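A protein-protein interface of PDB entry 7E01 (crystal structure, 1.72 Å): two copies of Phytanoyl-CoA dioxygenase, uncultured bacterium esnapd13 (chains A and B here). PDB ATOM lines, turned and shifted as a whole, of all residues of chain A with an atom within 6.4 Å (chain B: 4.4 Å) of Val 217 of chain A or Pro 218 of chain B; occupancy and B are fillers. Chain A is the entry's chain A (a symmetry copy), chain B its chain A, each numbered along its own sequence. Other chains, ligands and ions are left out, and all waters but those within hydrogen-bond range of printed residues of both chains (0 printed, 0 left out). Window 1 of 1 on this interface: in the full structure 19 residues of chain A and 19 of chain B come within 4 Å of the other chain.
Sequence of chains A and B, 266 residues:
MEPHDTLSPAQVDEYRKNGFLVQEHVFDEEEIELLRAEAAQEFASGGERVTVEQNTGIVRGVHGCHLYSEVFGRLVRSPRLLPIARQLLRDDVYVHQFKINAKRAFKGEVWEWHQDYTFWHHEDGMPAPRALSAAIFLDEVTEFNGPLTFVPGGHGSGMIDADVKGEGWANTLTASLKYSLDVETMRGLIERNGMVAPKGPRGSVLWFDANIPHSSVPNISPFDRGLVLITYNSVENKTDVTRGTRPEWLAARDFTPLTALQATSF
O of Phe 144 of chain B is in hydrogen-bond range of N of Ile 220 of chain B (3.1 Å). O of Val 217 of chain A lies within hydrogen-bond range of NZ of Lys 103 of chain A (2.9 Å). OG1 of Thr 149 of chain A is in hydrogen-bond range of O of Pro 147 of chain A, at 3.1 Å. N of Thr 149 of chain A is in hydrogen-bond range of O of Ser 215 of chain A (2.7 Å).
Pro 218 of chain B touches Val 110 of chain A. Val 110 of chain A touches Ile 220 of chain B (CG1 to CG2, 3.7 Å). CG2 of Thr 149 of chain A touches CE1 of Phe 144 of chain B, at 3.7 Å. Pro 218 of chain B touches Val 217 of chain A (O to CG1, 3.98 Å). Val 217 of chain A touches Ile 220 of chain B. CG2 of Val 110 of chain B touches CG of Pro 218 of chain A, at 3.7 Å. CG1 of Val 217 of chain B touches O of Pro 218 of chain A, at 3.98 Å. Pro 218 of chain A touches Pro 218 of chain B.
Of the printed residues of chain B, Val 217 of chain A touches Pro 218 and Ile 220. Of the printed residues of chain A, Ile 220 of chain B touches Val 110 (3.7 Å) and Val 217 (3.4 Å). Of the printed residues of chain A, Phe 144 of chain B touches Thr 149 (3.7 Å). Asn 219 of chain B touches none of the printed residues of chain A. Glu 109 of chain B touches none of the printed residues of chain A. The nearest printed residue of chain B that does not touch Val 217 of chain A is Val 217 of chain B (4.2 Å). The nearest printed residue of chain A that does not touch Pro 218 of chain B is Glu 109 of chain A (6.9 Å). The nearest printed residue of chain A that does not touch Val 217 of chain B is Val 217 of chain A (4.2 Å).
Of the 10 printed residues of chain B, 5 touch a printed residue of chain A. Printed residues of chain B that touch a printed residue of chain A: Val 110, Phe 144, Val 217, Pro 218 and Ile 220. Hydrophobic or aromatic side chains of chain B within 4 Å of the printed part of chain A: Val 110, Phe 144, Val 217, Pro 218 and Ile 220. Among the printed residues, no Asp or Glu carboxylate lies within 4 Å of a Lys or Arg side-chain nitrogen of the other chain.
Val 110 of chain A touches Pro 218 of chain B, and with the chains exchanged Pro 218 of chain A touches Val 110 of chain B. Val 217 of chain A touches Pro 218 of chain B, and with the chains exchanged Pro 218 of chain A touches Val 217 of chain B. Pro 218 of chain A touches its own counterpart, Pro 218 of chain B. Positions printed for both chains: 107, 108, 109, 110, 144, 146, 217, 218 and 219. Of the 8 pairs that touch across the chains among the printed residues, 5 have their exchanged pair printed and touching as well.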
ATOM      1  N   LYS A 103      -8.143  -3.169  25.717  1.00  0.00           N
ATOM      2  CA  LYS A 103      -8.228  -1.704  25.444  1.00  0.00           C
ATOM      3  C   LYS A 103      -8.753  -1.135  26.628  1.00  0.00           C
ATOM      4  O   LYS A 103      -9.936  -1.294  26.864  1.00  0.00           O
ATOM      5  CB  LYS A 103      -9.183  -1.344  24.285  1.00  0.00           C
ATOM      6  CG  LYS A 103      -8.531  -1.503  22.941  1.00  0.00           C
ATOM      7  CD  LYS A 103      -9.509  -1.063  21.846  1.00  0.00           C
ATOM      8  CE  LYS A 103      -8.928  -1.343  20.483  1.00  0.00           C
ATOM      9  NZ  LYS A 103     -10.007  -1.153  19.501  1.00  0.00           N
ATOM     10  N   LYS A 107      -8.480   4.546  26.813  1.00  0.00           N
ATOM     11  CA  LYS A 107      -7.281   4.338  26.028  1.00  0.00           C
ATOM     12  C   LYS A 107      -7.670   3.657  24.695  1.00  0.00           C
ATOM     13  O   LYS A 107      -8.847   3.731  24.277  1.00  0.00           O
ATOM     14  CB  LYS A 107      -6.192   3.645  26.871  1.00  0.00           C
ATOM     15  CG  LYS A 107      -5.149   4.611  27.460  1.00  0.00           C
ATOM     16  CD  LYS A 107      -4.579   5.681  26.504  1.00  0.00           C
ATOM     17  CE  LYS A 107      -4.220   5.202  25.088  1.00  0.00           C
ATOM     18  NZ  LYS A 107      -3.452   3.899  24.941  1.00  0.00           N
ATOM     19  N   GLY A 108      -6.675   3.088  24.010  1.00  0.00           N
ATOM     20  CA  GLY A 108      -6.846   2.402  22.755  1.00  0.00           C
ATOM     21  C   GLY A 108      -6.268   3.129  21.577  1.00  0.00           C
ATOM     22  O   GLY A 108      -5.966   4.328  21.654  1.00  0.00           O
ATOM     23  N   GLU A 109      -6.163   2.382  20.464  1.00  0.00           N
ATOM     24  CA  GLU A 109      -5.704   2.883  19.152  1.00  0.00           C
ATOM     25  C   GLU A 109      -6.689   2.563  18.026  1.00  0.00           C
ATOM     26  O   GLU A 109      -7.530   1.651  18.138  1.00  0.00           O
ATOM     27  CB  GLU A 109      -4.327   2.302  18.765  1.00  0.00           C
ATOM     28  CG  GLU A 109      -4.281   0.789  18.605  1.00  0.00           C
ATOM     29  CD  GLU A 109      -4.281   0.087  19.947  1.00  0.00           C
ATOM     30  OE1 GLU A 109      -3.201   0.071  20.610  1.00  0.00           O
ATOM     31  OE2 GLU A 109      -5.373  -0.408  20.340  1.00  0.00           O
ATOM     32  N   VAL A 110      -6.562   3.327  16.936  1.00  0.00           N
ATOM     33  CA  VAL A 110      -7.116   2.936  15.626  1.00  0.00           C
ATOM     34  C   VAL A 110      -6.281   1.739  15.134  1.00  0.00           C
ATOM     35  O   VAL A 110      -5.084   1.902  14.987  1.00  0.00           O
ATOM     36  CB  VAL A 110      -6.994   4.068  14.552  1.00  0.00           C
ATOM     37  CG1 VAL A 110      -7.780   3.687  13.293  1.00  0.00           C
ATOM     38  CG2 VAL A 110      -7.424   5.440  15.111  1.00  0.00           C
ATOM     39  N   TRP A 111      -6.947   0.630  14.833  1.00  0.00           N
ATOM     40  CA  TRP A 111      -6.303  -0.524  14.254  1.00  0.00           C
ATOM     41  C   TRP A 111      -6.725  -0.574  12.872  1.00  0.00           C
ATOM     42  O   TRP A 111      -7.915  -0.771  12.546  1.00  0.00           O
ATOM     43  CB  TRP A 111      -6.759  -1.818  14.794  1.00  0.00           C
ATOM     44  CG  TRP A 111      -6.162  -2.149  16.077  1.00  0.00           C
ATOM     45  CD1 TRP A 111      -6.331  -1.472  17.261  1.00  0.00           C
ATOM     46  CD2 TRP A 111      -5.327  -3.288  16.390  1.00  0.00           C
ATOM     47  NE1 TRP A 111      -5.667  -2.093  18.266  1.00  0.00           N
ATOM     48  CE2 TRP A 111      -5.030  -3.188  17.803  1.00  0.00           C
ATOM     49  CE3 TRP A 111      -4.780  -4.311  15.665  1.00  0.00           C
ATOM     50  CZ2 TRP A 111      -4.249  -4.101  18.444  1.00  0.00           C
ATOM     51  CZ3 TRP A 111      -3.988  -5.216  16.321  1.00  0.00           C
ATOM     52  CH2 TRP A 111      -3.740  -5.119  17.682  1.00  0.00           C
ATOM     53  N   GLU A 143     -20.638   0.083  21.662  1.00  0.00           N
ATOM     54  CA  GLU A 143     -20.282   0.989  20.608  1.00  0.00           C
ATOM     55  C   GLU A 143     -19.069   1.799  20.888  1.00  0.00           C
ATOM     56  O   GLU A 143     -18.384   2.278  19.936  1.00  0.00           O
ATOM     57  CB  GLU A 143     -21.549   1.909  20.352  1.00  0.00           C
ATOM     58  CG  GLU A 143     -21.459   2.819  19.177  1.00  0.00           C
ATOM     59  CD  GLU A 143     -22.709   3.638  18.914  1.00  0.00           C
ATOM     60  OE1 GLU A 143     -23.805   3.409  19.416  1.00  0.00           O
ATOM     61  OE2 GLU A 143     -22.484   4.539  18.077  1.00  0.00           O
ATOM     62  N   PHE A 144     -18.736   1.982  22.189  1.00  0.00           N
ATOM     63  CA  PHE A 144     -17.791   2.944  22.596  1.00  0.00           C
ATOM     64  C   PHE A 144     -16.528   2.492  23.161  1.00  0.00           C
ATOM     65  O   PHE A 144     -15.691   3.288  23.442  1.00  0.00           O
ATOM     66  CB  PHE A 144     -18.498   3.959  23.601  1.00  0.00           C
ATOM     67  CG  PHE A 144     -19.849   4.345  23.176  1.00  0.00           C
ATOM     68  CD1 PHE A 144     -19.977   5.316  22.125  1.00  0.00           C
ATOM     69  CD2 PHE A 144     -20.971   3.828  23.702  1.00  0.00           C
ATOM     70  CE1 PHE A 144     -21.237   5.654  21.665  1.00  0.00           C
ATOM     71  CE2 PHE A 144     -22.239   4.168  23.264  1.00  0.00           C
ATOM     72  CZ  PHE A 144     -22.366   5.110  22.208  1.00  0.00           C
ATOM     73  N   ASN A 145     -16.239   1.168  23.289  1.00  0.00           N
ATOM     74  CA  ASN A 145     -14.945   0.796  23.771  1.00  0.00           C
ATOM     75  C   ASN A 145     -14.097   0.008  22.780  1.00  0.00           C
ATOM     76  O   ASN A 145     -13.297  -0.909  23.084  1.00  0.00           O
ATOM     77  CB  ASN A 145     -15.168  -0.093  25.034  1.00  0.00           C
ATOM     78  CG  ASN A 145     -16.043  -1.334  24.811  1.00  0.00           C
ATOM     79  OD1 ASN A 145     -16.601  -1.650  23.775  1.00  0.00           O
ATOM     80  ND2 ASN A 145     -16.187  -2.082  25.917  1.00  0.00           N
ATOM     81  N   GLY A 146     -14.198   0.478  21.546  1.00  0.00           N
ATOM     82  CA  GLY A 146     -13.321   0.030  20.509  1.00  0.00           C
ATOM     83  C   GLY A 146     -13.585  -1.382  19.980  1.00  0.00           C
ATOM     84  O   GLY A 146     -12.631  -2.151  19.853  1.00  0.00           O
ATOM     85  N   PRO A 147     -14.802  -1.689  19.707  1.00  0.00           N
ATOM     86  CA  PRO A 147     -15.085  -3.006  19.252  1.00  0.00           C
ATOM     87  C   PRO A 147     -14.459  -3.362  17.952  1.00  0.00           C
ATOM     88  O   PRO A 147     -14.255  -2.524  17.062  1.00  0.00           O
ATOM     89  CB  PRO A 147     -16.558  -3.022  19.135  1.00  0.00           C
ATOM     90  CG  PRO A 147     -16.931  -1.547  18.666  1.00  0.00           C
ATOM     91  CD  PRO A 147     -16.018  -0.847  19.591  1.00  0.00           C
ATOM     92  N   THR A 149     -14.554  -4.279  14.374  1.00  0.00           N
ATOM     93  CA  THR A 149     -15.402  -3.759  13.310  1.00  0.00           C
ATOM     94  C   THR A 149     -15.021  -4.439  11.947  1.00  0.00           C
ATOM     95  O   THR A 149     -13.900  -4.579  11.668  1.00  0.00           O
ATOM     96  CB  THR A 149     -15.302  -2.191  13.182  1.00  0.00           C
ATOM     97  OG1 THR A 149     -15.602  -1.638  14.468  1.00  0.00           O
ATOM     98  CG2 THR A 149     -16.316  -1.687  12.234  1.00  0.00           C
ATOM     99  N   SER A 215     -11.125  -3.989  11.795  1.00  0.00           N
ATOM    100  CA  SER A 215     -10.543  -2.715  12.252  1.00  0.00           C
ATOM    101  C   SER A 215     -11.197  -2.456  13.638  1.00  0.00           C
ATOM    102  O   SER A 215     -12.228  -3.061  14.014  1.00  0.00           O
ATOM    103  CB  SER A 215     -11.046  -1.566  11.328  1.00  0.00           C
ATOM    104  OG  SER A 215     -10.394  -0.300  11.514  1.00  0.00           O
ATOM    105  N   SER A 216     -10.620  -1.541  14.374  1.00  0.00           N
ATOM    106  CA  SER A 216     -11.299  -1.030  15.563  1.00  0.00           C
ATOM    107  C   SER A 216     -10.764   0.348  15.919  1.00  0.00           C
ATOM    108  O   SER A 216      -9.683   0.646  15.529  1.00  0.00           O
ATOM    109  CB  SER A 216     -11.019  -2.005  16.704  1.00  0.00           C
ATOM    110  OG  SER A 216      -9.616  -2.133  16.992  1.00  0.00           O
ATOM    111  N   VAL A 217     -11.507   1.128  16.694  1.00  0.00           N
ATOM    112  CA  VAL A 217     -11.074   2.514  17.109  1.00  0.00           C
ATOM    113  C   VAL A 217     -10.797   2.566  18.578  1.00  0.00           C
ATOM    114  O   VAL A 217     -10.999   1.551  19.253  1.00  0.00           O
ATOM    115  CB  VAL A 217     -12.181   3.520  16.855  1.00  0.00           C
ATOM    116  CG1 VAL A 217     -12.494   3.568  15.374  1.00  0.00           C
ATOM    117  CG2 VAL A 217     -13.449   3.177  17.635  1.00  0.00           C
ATOM    118  N   PRO A 218     -10.434   3.763  19.139  1.00  0.00           N
ATOM    119  CA  PRO A 218     -10.285   3.814  20.627  1.00  0.00           C
ATOM    120  C   PRO A 218     -11.448   3.710  21.547  1.00  0.00           C
ATOM    121  O   PRO A 218     -12.614   3.950  21.147  1.00  0.00           O
ATOM    122  CB  PRO A 218      -9.444   5.097  20.871  1.00  0.00           C
ATOM    123  CG  PRO A 218      -8.782   5.373  19.556  1.00  0.00           C
ATOM    124  CD  PRO A 218      -9.772   4.917  18.495  1.00  0.00           C
ATOM    125  N   ASN A 219     -11.171   3.194  22.778  1.00  0.00           N
ATOM    126  CA  ASN A 219     -12.158   3.124  23.865  1.00  0.00           C
ATOM    127  C   ASN A 219     -12.232   4.517  24.498  1.00  0.00           C
ATOM    128  O   ASN A 219     -11.302   4.971  25.149  1.00  0.00           O
ATOM    129  CB  ASN A 219     -11.667   2.129  24.919  1.00  0.00           C
ATOM    130  CG  ASN A 219     -12.645   1.871  25.999  1.00  0.00           C
ATOM    131  OD1 ASN A 219     -13.657   2.610  26.228  1.00  0.00           O
ATOM    132  ND2 ASN A 219     -12.343   0.792  26.782  1.00  0.00           N
ATOM    133  N   ARG A 225     -11.911  -2.982  27.452  1.00  0.00           N
ATOM    134  CA  ARG A 225     -12.333  -4.023  26.438  1.00  0.00           C
ATOM    135  C   ARG A 225     -11.312  -5.160  26.264  1.00  0.00           C
ATOM    136  O   ARG A 225     -10.502  -5.260  25.300  1.00  0.00           O
ATOM    137  CB  ARG A 225     -12.682  -3.368  25.099  1.00  0.00           C
ATOM    138  CG  ARG A 225     -13.425  -4.269  24.147  1.00  0.00           C
ATOM    139  CD  ARG A 225     -12.697  -4.223  22.818  1.00  0.00           C
ATOM    140  NE  ARG A 225     -11.361  -4.756  22.750  1.00  0.00           N
ATOM    141  CZ  ARG A 225     -10.622  -4.872  21.679  1.00  0.00           C
ATOM    142  NH1 ARG A 225     -11.003  -4.487  20.426  1.00  0.00           N
ATOM    143  NH2 ARG A 225      -9.439  -5.458  21.832  1.00  0.00           N
ATOM    144  N   LYS B 107      -9.592   9.310   8.453  1.00  0.00           N
ATOM    145  CA  LYS B 107      -8.821  10.200   9.297  1.00  0.00           C
ATOM    146  C   LYS B 107      -9.617  10.471  10.595  1.00  0.00           C
ATOM    147  O   LYS B 107     -10.516   9.678  10.952  1.00  0.00           O
ATOM    148  CB  LYS B 107      -8.351  11.433   8.499  1.00  0.00           C
ATOM    149  CG  LYS B 107      -6.905  11.329   7.983  1.00  0.00           C
ATOM    150  CD  LYS B 107      -5.847  10.824   8.987  1.00  0.00           C
ATOM    151  CE  LYS B 107      -5.935  11.396  10.411  1.00  0.00           C
ATOM    152  NZ  LYS B 107      -6.146  12.892  10.574  1.00  0.00           N
ATOM    153  N   GLY B 108      -9.224  11.521  11.320  1.00  0.00           N
ATOM    154  CA  GLY B 108      -9.848  11.931  12.552  1.00  0.00           C
ATOM    155  C   GLY B 108      -9.007  11.696  13.771  1.00  0.00           C
ATOM    156  O   GLY B 108      -8.025  10.941  13.732  1.00  0.00           O
ATOM    157  N   GLU B 109      -9.444  12.327  14.875  1.00  0.00           N
ATOM    158  CA  GLU B 109      -8.844  12.194  16.218  1.00  0.00           C
ATOM    159  C   GLU B 109      -9.873  11.816  17.284  1.00  0.00           C
ATOM    160  O   GLU B 109     -11.091  12.015  17.113  1.00  0.00           O
ATOM    161  CB  GLU B 109      -8.143  13.494  16.666  1.00  0.00           C
ATOM    162  CG  GLU B 109      -9.050  14.709  16.801  1.00  0.00           C
ATOM    163  CD  GLU B 109      -9.414  15.285  15.448  1.00  0.00           C
ATOM    164  OE1 GLU B 109      -8.542  15.978  14.842  1.00  0.00           O
ATOM    165  OE2 GLU B 109     -10.556  15.006  14.989  1.00  0.00           O
ATOM    166  N   VAL B 110      -9.358  11.275  18.394  1.00  0.00           N
ATOM    167  CA  VAL B 110     -10.103  11.215  19.665  1.00  0.00           C
ATOM    168  C   VAL B 110     -10.213  12.663  20.179  1.00  0.00           C
ATOM    169  O   VAL B 110      -9.181  13.272  20.391  1.00  0.00           O
ATOM    170  CB  VAL B 110      -9.364  10.382  20.765  1.00  0.00           C
ATOM    171  CG1 VAL B 110     -10.281  10.172  21.974  1.00  0.00           C
ATOM    172  CG2 VAL B 110      -8.823   9.048  20.209  1.00  0.00           C
ATOM    173  N   PHE B 144     -19.463   4.902  12.487  1.00  0.00           N
ATOM    174  CA  PHE B 144     -18.106   4.737  12.148  1.00  0.00           C
ATOM    175  C   PHE B 144     -17.365   5.884  11.642  1.00  0.00           C
ATOM    176  O   PHE B 144     -16.202   5.780  11.419  1.00  0.00           O
ATOM    177  CB  PHE B 144     -17.980   3.520  11.126  1.00  0.00           C
ATOM    178  CG  PHE B 144     -18.823   2.374  11.486  1.00  0.00           C
ATOM    179  CD1 PHE B 144     -18.379   1.513  12.546  1.00  0.00           C
ATOM    180  CD2 PHE B 144     -19.996   2.097  10.893  1.00  0.00           C
ATOM    181  CE1 PHE B 144     -19.182   0.460  12.946  1.00  0.00           C
ATOM    182  CE2 PHE B 144     -20.803   1.038  11.270  1.00  0.00           C
ATOM    183  CZ  PHE B 144     -20.375   0.201  12.335  1.00  0.00           C
ATOM    184  N   GLY B 146     -16.867   8.877  13.340  1.00  0.00           N
ATOM    185  CA  GLY B 146     -16.510   9.752  14.412  1.00  0.00           C
ATOM    186  C   GLY B 146     -17.617  10.689  14.901  1.00  0.00           C
ATOM    187  O   GLY B 146     -17.351  11.881  15.064  1.00  0.00           O
ATOM    188  N   VAL B 217     -14.608   9.941  18.337  1.00  0.00           N
ATOM    189  CA  VAL B 217     -13.390   9.128  17.970  1.00  0.00           C
ATOM    190  C   VAL B 217     -13.064   9.285  16.519  1.00  0.00           C
ATOM    191  O   VAL B 217     -13.814   9.970  15.816  1.00  0.00           O
ATOM    192  CB  VAL B 217     -13.650   7.648  18.183  1.00  0.00           C
ATOM    193  CG1 VAL B 217     -13.944   7.390  19.647  1.00  0.00           C
ATOM    194  CG2 VAL B 217     -14.816   7.148  17.333  1.00  0.00           C
ATOM    195  N   PRO B 218     -12.010   8.578  15.999  1.00  0.00           N
ATOM    196  CA  PRO B 218     -11.784   8.658  14.522  1.00  0.00           C
ATOM    197  C   PRO B 218     -12.712   8.037  13.541  1.00  0.00           C
ATOM    198  O   PRO B 218     -13.499   7.120  13.884  1.00  0.00           O
ATOM    199  CB  PRO B 218     -10.318   8.174  14.346  1.00  0.00           C
ATOM    200  CG  PRO B 218      -9.697   8.342  15.699  1.00  0.00           C
ATOM    201  CD  PRO B 218     -10.811   8.068  16.698  1.00  0.00           C
ATOM    202  N   ASN B 219     -12.749   8.636  12.317  1.00  0.00           N
ATOM    203  CA  ASN B 219     -13.510   8.101  11.178  1.00  0.00           C
ATOM    204  C   ASN B 219     -12.674   6.972  10.568  1.00  0.00           C
ATOM    205  O   ASN B 219     -11.630   7.202   9.975  1.00  0.00           O
ATOM    206  CB  ASN B 219     -13.685   9.205  10.134  1.00  0.00           C
ATOM    207  CG  ASN B 219     -14.555   8.823   9.000  1.00  0.00           C
ATOM    208  OD1 ASN B 219     -14.880   7.620   8.731  1.00  0.00           O
ATOM    209  ND2 ASN B 219     -14.943   9.871   8.215  1.00  0.00           N
ATOM    210  N   ILE B 220     -13.125   5.737  10.757  1.00  0.00           N
ATOM    211  CA  ILE B 220     -12.471   4.568  10.112  1.00  0.00           C
ATOM    212  C   ILE B 220     -13.285   4.163   8.862  1.00  0.00           C
ATOM    213  O   ILE B 220     -13.090   3.055   8.264  1.00  0.00           O
ATOM    214  CB  ILE B 220     -12.349   3.382  11.132  1.00  0.00           C
ATOM    215  CG1 ILE B 220     -13.731   3.025  11.742  1.00  0.00           C
ATOM    216  CG2 ILE B 220     -11.328   3.743  12.196  1.00  0.00           C
ATOM    217  CD1 ILE B 220     -13.941   1.578  12.162  1.00  0.00           C
